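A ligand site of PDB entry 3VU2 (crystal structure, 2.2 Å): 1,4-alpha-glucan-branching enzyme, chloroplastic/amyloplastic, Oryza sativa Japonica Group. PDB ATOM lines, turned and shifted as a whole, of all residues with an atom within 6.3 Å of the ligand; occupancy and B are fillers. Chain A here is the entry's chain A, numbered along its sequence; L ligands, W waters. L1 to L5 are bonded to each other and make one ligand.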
ATOM      1  N   LEU A  40      -7.627 -32.843  26.491  1.00  0.00           N
ATOM      2  CA  LEU A  40      -6.311 -32.358  26.079  1.00  0.00           C
ATOM      3  C   LEU A  40      -5.822 -31.180  26.923  1.00  0.00           C
ATOM      4  O   LEU A  40      -4.622 -31.072  27.194  1.00  0.00           O
ATOM      5  CB  LEU A  40      -6.318 -31.971  24.599  1.00  0.00           C
ATOM      6  CG  LEU A  40      -6.406 -33.089  23.548  1.00  0.00           C
ATOM      7  CD1 LEU A  40      -6.879 -32.524  22.211  1.00  0.00           C
ATOM      8  CD2 LEU A  40      -5.085 -33.831  23.392  1.00  0.00           C
ATOM      9  N   LYS A  43      -4.812 -32.829  30.390  1.00  0.00           N
ATOM     10  CA  LYS A  43      -3.523 -33.519  30.349  1.00  0.00           C
ATOM     11  C   LYS A  43      -2.346 -32.569  30.212  1.00  0.00           C
ATOM     12  O   LYS A  43      -1.347 -32.726  30.914  1.00  0.00           O
ATOM     13  CB  LYS A  43      -3.481 -34.545  29.205  1.00  0.00           C
ATOM     14  CG  LYS A  43      -4.459 -35.696  29.352  1.00  0.00           C
ATOM     15  CD  LYS A  43      -4.064 -36.879  28.479  1.00  0.00           C
ATOM     16  CE  LYS A  43      -5.079 -38.006  28.580  1.00  0.00           C
ATOM     17  NZ  LYS A  43      -5.403 -38.367  30.014  1.00  0.00           N
ATOM     18  N   HIS A  44      -2.465 -31.581  29.328  1.00  0.00           N
ATOM     19  CA  HIS A  44      -1.310 -30.765  28.920  1.00  0.00           C
ATOM     20  C   HIS A  44      -1.234 -29.367  29.532  1.00  0.00           C
ATOM     21  O   HIS A  44      -0.203 -28.688  29.404  1.00  0.00           O
ATOM     22  CB  HIS A  44      -1.225 -30.712  27.393  1.00  0.00           C
ATOM     23  CG  HIS A  44      -1.314 -32.065  26.734  1.00  0.00           C
ATOM     24  ND1 HIS A  44      -0.266 -32.965  26.748  1.00  0.00           N
ATOM     25  CD2 HIS A  44      -2.319 -32.668  26.074  1.00  0.00           C
ATOM     26  CE1 HIS A  44      -0.631 -34.058  26.103  1.00  0.00           C
ATOM     27  NE2 HIS A  44      -1.874 -33.914  25.686  1.00  0.00           N
ATOM     28  N   GLU A  45      -2.296 -28.940  30.209  1.00  0.00           N
ATOM     29  CA  GLU A  45      -2.350 -27.571  30.776  1.00  0.00           C
ATOM     30  C   GLU A  45      -2.832 -27.528  32.231  1.00  0.00           C
ATOM     31  O   GLU A  45      -2.924 -26.443  32.816  1.00  0.00           O
ATOM     32  CB  GLU A  45      -3.222 -26.671  29.903  1.00  0.00           C
ATOM     33  CG  GLU A  45      -2.684 -26.441  28.484  1.00  0.00           C
ATOM     34  CD  GLU A  45      -1.606 -25.362  28.412  1.00  0.00           C
ATOM     35  OE1 GLU A  45      -1.246 -24.789  29.453  1.00  0.00           O
ATOM     36  OE2 GLU A  45      -1.124 -25.087  27.295  1.00  0.00           O
ATOM     37  N   PHE A  51      -5.589 -23.533  33.049  1.00  0.00           N
ATOM     38  CA  PHE A  51      -5.432 -23.017  31.691  1.00  0.00           C
ATOM     39  C   PHE A  51      -5.858 -21.542  31.590  1.00  0.00           C
ATOM     40  O   PHE A  51      -5.283 -20.775  30.813  1.00  0.00           O
ATOM     41  CB  PHE A  51      -6.235 -23.890  30.722  1.00  0.00           C
ATOM     42  CG  PHE A  51      -5.935 -23.650  29.259  1.00  0.00           C
ATOM     43  CD1 PHE A  51      -4.623 -23.527  28.803  1.00  0.00           C
ATOM     44  CD2 PHE A  51      -6.975 -23.590  28.340  1.00  0.00           C
ATOM     45  CE1 PHE A  51      -4.352 -23.326  27.454  1.00  0.00           C
ATOM     46  CE2 PHE A  51      -6.712 -23.385  26.980  1.00  0.00           C
ATOM     47  CZ  PHE A  51      -5.404 -23.261  26.546  1.00  0.00           C
ATOM     48  N   TRP A  72       2.662 -14.296  22.267  1.00  0.00           N
ATOM     49  CA  TRP A  72       2.470 -15.221  21.164  1.00  0.00           C
ATOM     50  C   TRP A  72       2.446 -14.449  19.850  1.00  0.00           C
ATOM     51  O   TRP A  72       1.580 -13.582  19.640  1.00  0.00           O
ATOM     52  CB  TRP A  72       1.156 -15.980  21.361  1.00  0.00           C
ATOM     53  CG  TRP A  72       0.862 -17.054  20.346  1.00  0.00           C
ATOM     54  CD1 TRP A  72       1.595 -18.177  20.109  1.00  0.00           C
ATOM     55  CD2 TRP A  72      -0.279 -17.113  19.472  1.00  0.00           C
ATOM     56  NE1 TRP A  72       0.997 -18.931  19.122  1.00  0.00           N
ATOM     57  CE2 TRP A  72      -0.152 -18.301  18.714  1.00  0.00           C
ATOM     58  CE3 TRP A  72      -1.378 -16.276  19.252  1.00  0.00           C
ATOM     59  CZ2 TRP A  72      -1.089 -18.672  17.749  1.00  0.00           C
ATOM     60  CZ3 TRP A  72      -2.309 -16.655  18.289  1.00  0.00           C
ATOM     61  CH2 TRP A  72      -2.163 -17.835  17.558  1.00  0.00           C
ATOM     62  N   PRO A  74       3.836 -16.235  16.330  1.00  0.00           N
ATOM     63  CA  PRO A  74       4.585 -17.257  15.585  1.00  0.00           C
ATOM     64  C   PRO A  74       5.122 -16.741  14.248  1.00  0.00           C
ATOM     65  O   PRO A  74       6.119 -17.253  13.738  1.00  0.00           O
ATOM     66  CB  PRO A  74       3.530 -18.328  15.309  1.00  0.00           C
ATOM     67  CG  PRO A  74       2.455 -18.089  16.278  1.00  0.00           C
ATOM     68  CD  PRO A  74       2.426 -16.618  16.484  1.00  0.00           C
ATOM     69  N   ALA A  75       4.456 -15.722  13.710  1.00  0.00           N
ATOM     70  CA  ALA A  75       4.782 -15.185  12.385  1.00  0.00           C
ATOM     71  C   ALA A  75       5.998 -14.255  12.367  1.00  0.00           C
ATOM     72  O   ALA A  75       6.614 -14.062  11.324  1.00  0.00           O
ATOM     73  CB  ALA A  75       3.559 -14.484  11.803  1.00  0.00           C
ATOM     74  N   LYS A  97      12.091 -16.749  20.838  1.00  0.00           N
ATOM     75  CA  LYS A  97      10.945 -17.522  20.386  1.00  0.00           C
ATOM     76  C   LYS A  97      11.087 -18.989  20.781  1.00  0.00           C
ATOM     77  O   LYS A  97      12.147 -19.593  20.573  1.00  0.00           O
ATOM     78  CB  LYS A  97      10.854 -17.392  18.868  1.00  0.00           C
ATOM     79  CG  LYS A  97       9.584 -17.887  18.218  1.00  0.00           C
ATOM     80  CD  LYS A  97       9.775 -17.926  16.708  1.00  0.00           C
ATOM     81  CE  LYS A  97       8.475 -18.040  15.962  1.00  0.00           C
ATOM     82  NZ  LYS A  97       8.691 -17.901  14.493  1.00  0.00           N
ATOM     83  N   ASP A  98      10.036 -19.554  21.365  1.00  0.00           N
ATOM     84  CA  ASP A  98       9.998 -20.977  21.696  1.00  0.00           C
ATOM     85  C   ASP A  98       9.364 -21.784  20.552  1.00  0.00           C
ATOM     86  O   ASP A  98       8.941 -21.209  19.546  1.00  0.00           O
ATOM     87  CB  ASP A  98       9.324 -21.225  23.077  1.00  0.00           C
ATOM     88  CG  ASP A  98       7.797 -21.149  23.035  1.00  0.00           C
ATOM     89  OD1 ASP A  98       7.198 -20.916  21.960  1.00  0.00           O
ATOM     90  OD2 ASP A  98       7.165 -21.323  24.106  1.00  0.00           O
ATOM     91  N   LYS A  99       9.291 -23.114  20.716  1.00  0.00           N
ATOM     92  CA  LYS A  99       8.805 -24.015  19.658  1.00  0.00           C
ATOM     93  C   LYS A  99       7.343 -23.768  19.226  1.00  0.00           C
ATOM     94  O   LYS A  99       6.900 -24.264  18.191  1.00  0.00           O
ATOM     95  CB  LYS A  99       9.002 -25.488  20.047  1.00  0.00           C
ATOM     96  CG  LYS A  99       8.414 -25.897  21.397  1.00  0.00           C
ATOM     97  CD  LYS A  99       8.708 -27.364  21.739  1.00  0.00           C
ATOM     98  CE  LYS A  99       7.675 -28.316  21.130  1.00  0.00           C
ATOM     99  NZ  LYS A  99       8.124 -29.750  21.202  1.00  0.00           N
ATOM    100  N   PHE A 100       6.622 -23.001  20.045  1.00  0.00           N
ATOM    101  CA  PHE A 100       5.215 -22.696  19.788  1.00  0.00           C
ATOM    102  C   PHE A 100       5.000 -21.286  19.241  1.00  0.00           C
ATOM    103  O   PHE A 100       3.872 -20.844  19.046  1.00  0.00           O
ATOM    104  CB  PHE A 100       4.393 -22.903  21.079  1.00  0.00           C
ATOM    105  CG  PHE A 100       4.468 -24.297  21.641  1.00  0.00           C
ATOM    106  CD1 PHE A 100       4.125 -25.397  20.877  1.00  0.00           C
ATOM    107  CD2 PHE A 100       4.875 -24.493  22.965  1.00  0.00           C
ATOM    108  CE1 PHE A 100       4.186 -26.689  21.405  1.00  0.00           C
ATOM    109  CE2 PHE A 100       4.938 -25.781  23.503  1.00  0.00           C
ATOM    110  CZ  PHE A 100       4.600 -26.882  22.717  1.00  0.00           C
ATOM    111  N   GLY A 101       6.103 -20.573  18.994  1.00  0.00           N
ATOM    112  CA  GLY A 101       6.028 -19.188  18.510  1.00  0.00           C
ATOM    113  C   GLY A 101       5.653 -18.208  19.601  1.00  0.00           C
ATOM    114  O   GLY A 101       5.097 -17.142  19.319  1.00  0.00           O
ATOM    115  N   ILE A 102       5.925 -18.579  20.846  1.00  0.00           N
ATOM    116  CA  ILE A 102       5.723 -17.692  21.987  1.00  0.00           C
ATOM    117  C   ILE A 102       7.039 -16.960  22.258  1.00  0.00           C
ATOM    118  O   ILE A 102       8.081 -17.592  22.468  1.00  0.00           O
ATOM    119  CB  ILE A 102       5.261 -18.468  23.243  1.00  0.00           C
ATOM    120  CG1 ILE A 102       3.943 -19.207  22.953  1.00  0.00           C
ATOM    121  CG2 ILE A 102       5.122 -17.528  24.442  1.00  0.00           C
ATOM    122  CD1 ILE A 102       3.465 -20.134  24.083  1.00  0.00           C
ATOM    123  N   HIS A 294      -3.739 -21.123  11.750  1.00  0.00           N
ATOM    124  CA  HIS A 294      -3.232 -21.892  12.886  1.00  0.00           C
ATOM    125  C   HIS A 294      -2.281 -21.063  13.742  1.00  0.00           C
ATOM    126  O   HIS A 294      -2.194 -21.266  14.955  1.00  0.00           O
ATOM    127  CB  HIS A 294      -2.545 -23.180  12.392  1.00  0.00           C
ATOM    128  CG  HIS A 294      -2.410 -24.238  13.437  1.00  0.00           C
ATOM    129  ND1 HIS A 294      -1.189 -24.570  13.998  1.00  0.00           N
ATOM    130  CD2 HIS A 294      -3.325 -25.048  14.022  1.00  0.00           C
ATOM    131  CE1 HIS A 294      -1.367 -25.533  14.883  1.00  0.00           C
ATOM    132  NE2 HIS A 294      -2.645 -25.841  14.918  1.00  0.00           N
ATOM    133  N   GLU A 295      -1.590 -20.107  13.117  1.00  0.00           N
ATOM    134  CA  GLU A 295      -0.663 -19.203  13.801  1.00  0.00           C
ATOM    135  C   GLU A 295      -1.244 -17.795  14.002  1.00  0.00           C
ATOM    136  O   GLU A 295      -0.498 -16.817  14.163  1.00  0.00           O
ATOM    137  CB  GLU A 295       0.677 -19.135  13.050  1.00  0.00           C
ATOM    138  CG  GLU A 295       1.600 -20.334  13.293  1.00  0.00           C
ATOM    139  CD  GLU A 295       1.131 -21.597  12.594  1.00  0.00           C
ATOM    140  OE1 GLU A 295       0.946 -22.624  13.279  1.00  0.00           O
ATOM    141  OE2 GLU A 295       0.936 -21.559  11.358  1.00  0.00           O
ATOM    142  N   TRP A 319      -5.477 -23.340  20.021  1.00  0.00           N
ATOM    143  CA  TRP A 319      -5.099 -23.531  21.412  1.00  0.00           C
ATOM    144  C   TRP A 319      -4.842 -22.207  22.131  1.00  0.00           C
ATOM    145  O   TRP A 319      -5.383 -21.965  23.204  1.00  0.00           O
ATOM    146  CB  TRP A 319      -3.846 -24.390  21.479  1.00  0.00           C
ATOM    147  CG  TRP A 319      -3.565 -24.957  22.833  1.00  0.00           C
ATOM    148  CD1 TRP A 319      -2.943 -24.344  23.876  1.00  0.00           C
ATOM    149  CD2 TRP A 319      -3.894 -26.281  23.290  1.00  0.00           C
ATOM    150  NE1 TRP A 319      -2.866 -25.190  24.952  1.00  0.00           N
ATOM    151  CE2 TRP A 319      -3.441 -26.395  24.622  1.00  0.00           C
ATOM    152  CE3 TRP A 319      -4.527 -27.380  22.695  1.00  0.00           C
ATOM    153  CZ2 TRP A 319      -3.599 -27.559  25.371  1.00  0.00           C
ATOM    154  CZ3 TRP A 319      -4.686 -28.544  23.445  1.00  0.00           C
ATOM    155  CH2 TRP A 319      -4.229 -28.618  24.763  1.00  0.00           C
ATOM    156  N   GLU A 320      -4.012 -21.368  21.526  1.00  0.00           N
ATOM    157  CA  GLU A 320      -3.685 -20.066  22.115  1.00  0.00           C
ATOM    158  C   GLU A 320      -4.878 -19.116  22.104  1.00  0.00           C
ATOM    159  O   GLU A 320      -4.915 -18.176  22.904  1.00  0.00           O
ATOM    160  CB  GLU A 320      -2.467 -19.433  21.420  1.00  0.00           C
ATOM    161  CG  GLU A 320      -1.120 -20.083  21.753  1.00  0.00           C
ATOM    162  CD  GLU A 320      -0.793 -20.124  23.238  1.00  0.00           C
ATOM    163  OE1 GLU A 320      -1.143 -19.175  23.972  1.00  0.00           O
ATOM    164  OE2 GLU A 320      -0.169 -21.122  23.678  1.00  0.00           O
ATOM    165  N   ARG A 323      -6.785 -20.279  25.190  1.00  0.00           N
ATOM    166  CA  ARG A 323      -6.108 -19.748  26.372  1.00  0.00           C
ATOM    167  C   ARG A 323      -6.417 -18.268  26.562  1.00  0.00           C
ATOM    168  O   ARG A 323      -6.681 -17.831  27.676  1.00  0.00           O
ATOM    169  CB  ARG A 323      -4.595 -19.947  26.277  1.00  0.00           C
ATOM    170  CG  ARG A 323      -3.880 -19.702  27.596  1.00  0.00           C
ATOM    171  CD  ARG A 323      -2.422 -19.345  27.379  1.00  0.00           C
ATOM    172  NE  ARG A 323      -1.711 -20.376  26.622  1.00  0.00           N
ATOM    173  CZ  ARG A 323      -1.239 -21.504  27.130  1.00  0.00           C
ATOM    174  NH1 ARG A 323      -1.407 -21.804  28.413  1.00  0.00           N
ATOM    175  NH2 ARG A 323      -0.606 -22.368  26.336  1.00  0.00           N
HETATM  176  C1  LIG L   1       5.807 -24.487  13.049  1.00  0.00           C
HETATM  177  C2  LIG L   1       5.347 -25.689  13.898  1.00  0.00           C
HETATM  178  C3  LIG L   1       4.268 -25.359  14.932  1.00  0.00           C
HETATM  179  C4  LIG L   1       4.468 -23.988  15.600  1.00  0.00           C
HETATM  180  C5  LIG L   1       4.706 -22.906  14.536  1.00  0.00           C
HETATM  181  C6  LIG L   1       4.909 -21.529  15.159  1.00  0.00           C
HETATM  182  O1  LIG L   1       4.961 -24.340  11.890  1.00  0.00           O
HETATM  183  O2  LIG L   1       4.851 -26.728  13.039  1.00  0.00           O
HETATM  184  O3  LIG L   1       4.290 -26.374  15.946  1.00  0.00           O
HETATM  185  O4  LIG L   1       3.434 -23.637  16.556  1.00  0.00           O
HETATM  186  O5  LIG L   1       5.869 -23.260  13.787  1.00  0.00           O
HETATM  187  O6  LIG L   1       6.269 -21.344  15.573  1.00  0.00           O
HETATM  188  C1  LG2 L   2       2.052 -23.651  16.151  1.00  0.00           C
HETATM  189  C2  LG2 L   2       1.255 -22.627  16.976  1.00  0.00           C
HETATM  190  C3  LG2 L   2       1.225 -23.019  18.454  1.00  0.00           C
HETATM  191  C4  LG2 L   2       0.756 -24.456  18.649  1.00  0.00           C
HETATM  192  C5  LG2 L   2       1.587 -25.374  17.749  1.00  0.00           C
HETATM  193  C6  LG2 L   2       1.225 -26.859  17.860  1.00  0.00           C
HETATM  194  O1  LG2 L   2       1.829 -21.325  16.845  1.00  0.00           O
HETATM  195  O2  LG2 L   2       0.383 -22.098  19.172  1.00  0.00           O
HETATM  196  O3  LG2 L   2       0.916 -24.844  20.012  1.00  0.00           O
HETATM  197  O4  LG2 L   2       1.474 -24.948  16.377  1.00  0.00           O
HETATM  198  O5  LG2 L   2      -0.103 -27.074  17.367  1.00  0.00           O
HETATM  199  C1  LG3 L   3      -0.278 -24.670  20.796  1.00  0.00           C
HETATM  200  C2  LG3 L   3       0.062 -23.949  22.099  1.00  0.00           C
HETATM  201  C3  LG3 L   3       0.884 -24.839  23.029  1.00  0.00           C
HETATM  202  C4  LG3 L   3       0.228 -26.212  23.218  1.00  0.00           C
HETATM  203  C5  LG3 L   3      -0.092 -26.835  21.857  1.00  0.00           C
HETATM  204  C6  LG3 L   3      -0.835 -28.165  21.979  1.00  0.00           C
HETATM  205  O1  LG3 L   3       0.796 -22.754  21.833  1.00  0.00           O
HETATM  206  O2  LG3 L   3       1.077 -24.185  24.302  1.00  0.00           O
HETATM  207  O3  LG3 L   3       1.171 -27.024  23.911  1.00  0.00           O
HETATM  208  O4  LG3 L   3      -0.891 -25.933  21.069  1.00  0.00           O
HETATM  209  O5  LG3 L   3      -0.863 -28.821  20.716  1.00  0.00           O
HETATM  210  C1  LG4 L   4       0.680 -27.593  25.132  1.00  0.00           C
HETATM  211  C2  LG4 L   4       1.499 -27.085  26.323  1.00  0.00           C
HETATM  212  C3  LG4 L   4       2.962 -27.473  26.173  1.00  0.00           C
HETATM  213  C4  LG4 L   4       3.144 -28.966  25.877  1.00  0.00           C
HETATM  214  C5  LG4 L   4       2.161 -29.467  24.815  1.00  0.00           C
HETATM  215  C6  LG4 L   4       2.140 -30.992  24.741  1.00  0.00           C
HETATM  216  O1  LG4 L   4       1.375 -25.664  26.432  1.00  0.00           O
HETATM  217  O2  LG4 L   4       3.662 -27.133  27.375  1.00  0.00           O
HETATM  218  O3  LG4 L   4       4.489 -29.189  25.430  1.00  0.00           O
HETATM  219  O4  LG4 L   4       0.822 -29.016  25.063  1.00  0.00           O
HETATM  220  O5  LG4 L   4       1.736 -31.527  26.012  1.00  0.00           O
HETATM  221  C1  LG5 L   5       5.306 -29.904  26.386  1.00  0.00           C
HETATM  222  C2  LG5 L   5       6.725 -29.330  26.388  1.00  0.00           C
HETATM  223  C3  LG5 L   5       7.440 -29.650  25.071  1.00  0.00           C
HETATM  224  C4  LG5 L   5       7.392 -31.153  24.780  1.00  0.00           C
HETATM  225  C5  LG5 L   5       5.950 -31.667  24.835  1.00  0.00           C
HETATM  226  C6  LG5 L   5       5.863 -33.179  24.659  1.00  0.00           C
HETATM  227  O1  LG5 L   5       6.675 -27.907  26.582  1.00  0.00           O
HETATM  228  O2  LG5 L   5       8.799 -29.210  25.128  1.00  0.00           O
HETATM  229  O3  LG5 L   5       7.960 -31.406  23.493  1.00  0.00           O
HETATM  230  O4  LG5 L   5       5.333 -31.305  26.080  1.00  0.00           O
HETATM  231  O5  LG5 L   5       4.494 -33.613  24.783  1.00  0.00           O
HETATM  232  O   HOH W   1      -2.448 -22.058  19.223  1.00  0.00           O
HETATM  233  O   HOH W   2       2.805 -22.917  25.962  1.00  0.00           O
HETATM  234  O   HOH W   3      -2.276 -27.066  19.045  1.00  0.00           O
HETATM  235  O   HOH W   4      -1.887 -31.204  22.914  1.00  0.00           O
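An oxygen (O2) of LG2 L2 sits at hydrogen-bond distance from the indole nitrogen (NE1) of Trp 72 (3.2 Å).
O of Phe 100 sits at hydrogen-bond distance from O1 of LG2 L2 (3.0 Å).
The side-chain carboxylate (OE2) of Glu 45 lies within hydrogen-bond range of an oxygen (O1) of LG4 L4.
OE2 of Glu 320 lies within hydrogen-bond range of O1 of LG3 L3, at 2.6 Å.
A ring nitrogen (ND1) of His 44 lies within hydrogen-bond range of an oxygen (O5) of LG4 L4, at 2.6 Å.
NH2 of Arg 323 is in hydrogen-bond range of O2 of LG3 L3, at 3.2 Å.
NZ of Lys 99 sits at hydrogen-bond distance from O3 of LG5 L5, at 2.8 Å.
The backbone carbonyl oxygen of Pro 74 sits at hydrogen-bond distance from the side-chain amino group of Lys 97 (2.8 Å).
The side-chain carboxylate of Asp 98 is in hydrogen-bond range of the backbone NH of Phe 100 (2.9 Å).
The side-chain carboxylate (OD1) of Asp 98 sits at hydrogen-bond distance from the backbone NH (N) of Gly 101, 3.2 Å away.
The guanidinium group (NE) of Arg 323 lies within salt-bridge range of the side-chain carboxylate (OE1) of Glu 320, at 3.0 Å.
The side-chain carboxylate (OE2) of Glu 45 is in hydrogen-bond range of the indole nitrogen (NE1) of Trp 319, at 2.9 Å.
ND1 of His 294 lies within hydrogen-bond range of OE1 of Glu 295 (3.0 Å).
The side-chain carboxylate (OE2) of Glu 45 lies within salt-bridge range of the guanidinium group (NH2) of Arg 323, 2.9 Å away.
The backbone carbonyl oxygen (O) of Phe 100 is in hydrogen-bond range of the indole nitrogen (NE1) of Trp 72.
Merely in contact with the ligand: His 294 (3.2 Å), Glu 295 (3.2 Å), Pro 74 (3.3 Å), Trp 319 (3.3 Å), Gly 101 (3.5 Å) and Lys 97 (3.99 Å).
Hydrophobic or aromatic side chains that line the ligand: His 44, Trp 72, Pro 74, Phe 100, His 294 and Trp 319.
13 residues have an atom within 4 Å of the ligand: His 44, Glu 45, Trp 72, Pro 74, Lys 97, Lys 99, Phe 100, Gly 101, His 294, Glu 295, Trp 319, Glu 320 and Arg 323.
Along chain A the residues within 4 Å of the ligand span positions 44 to 323.
The nearest printed residue that does not touch the ligand is Ile 102 (4.4 Å).
Water W2 bridges an oxygen (O2) of LG3 L3 (2.7 Å) and the guanidinium group (NH2) of Arg 323 (3.5 Å).
Water W1 lies within hydrogen-bond range of an oxygen (O2) of LG2 L2, the backbone NH of Glu 320 and the backbone NH of Trp 319.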
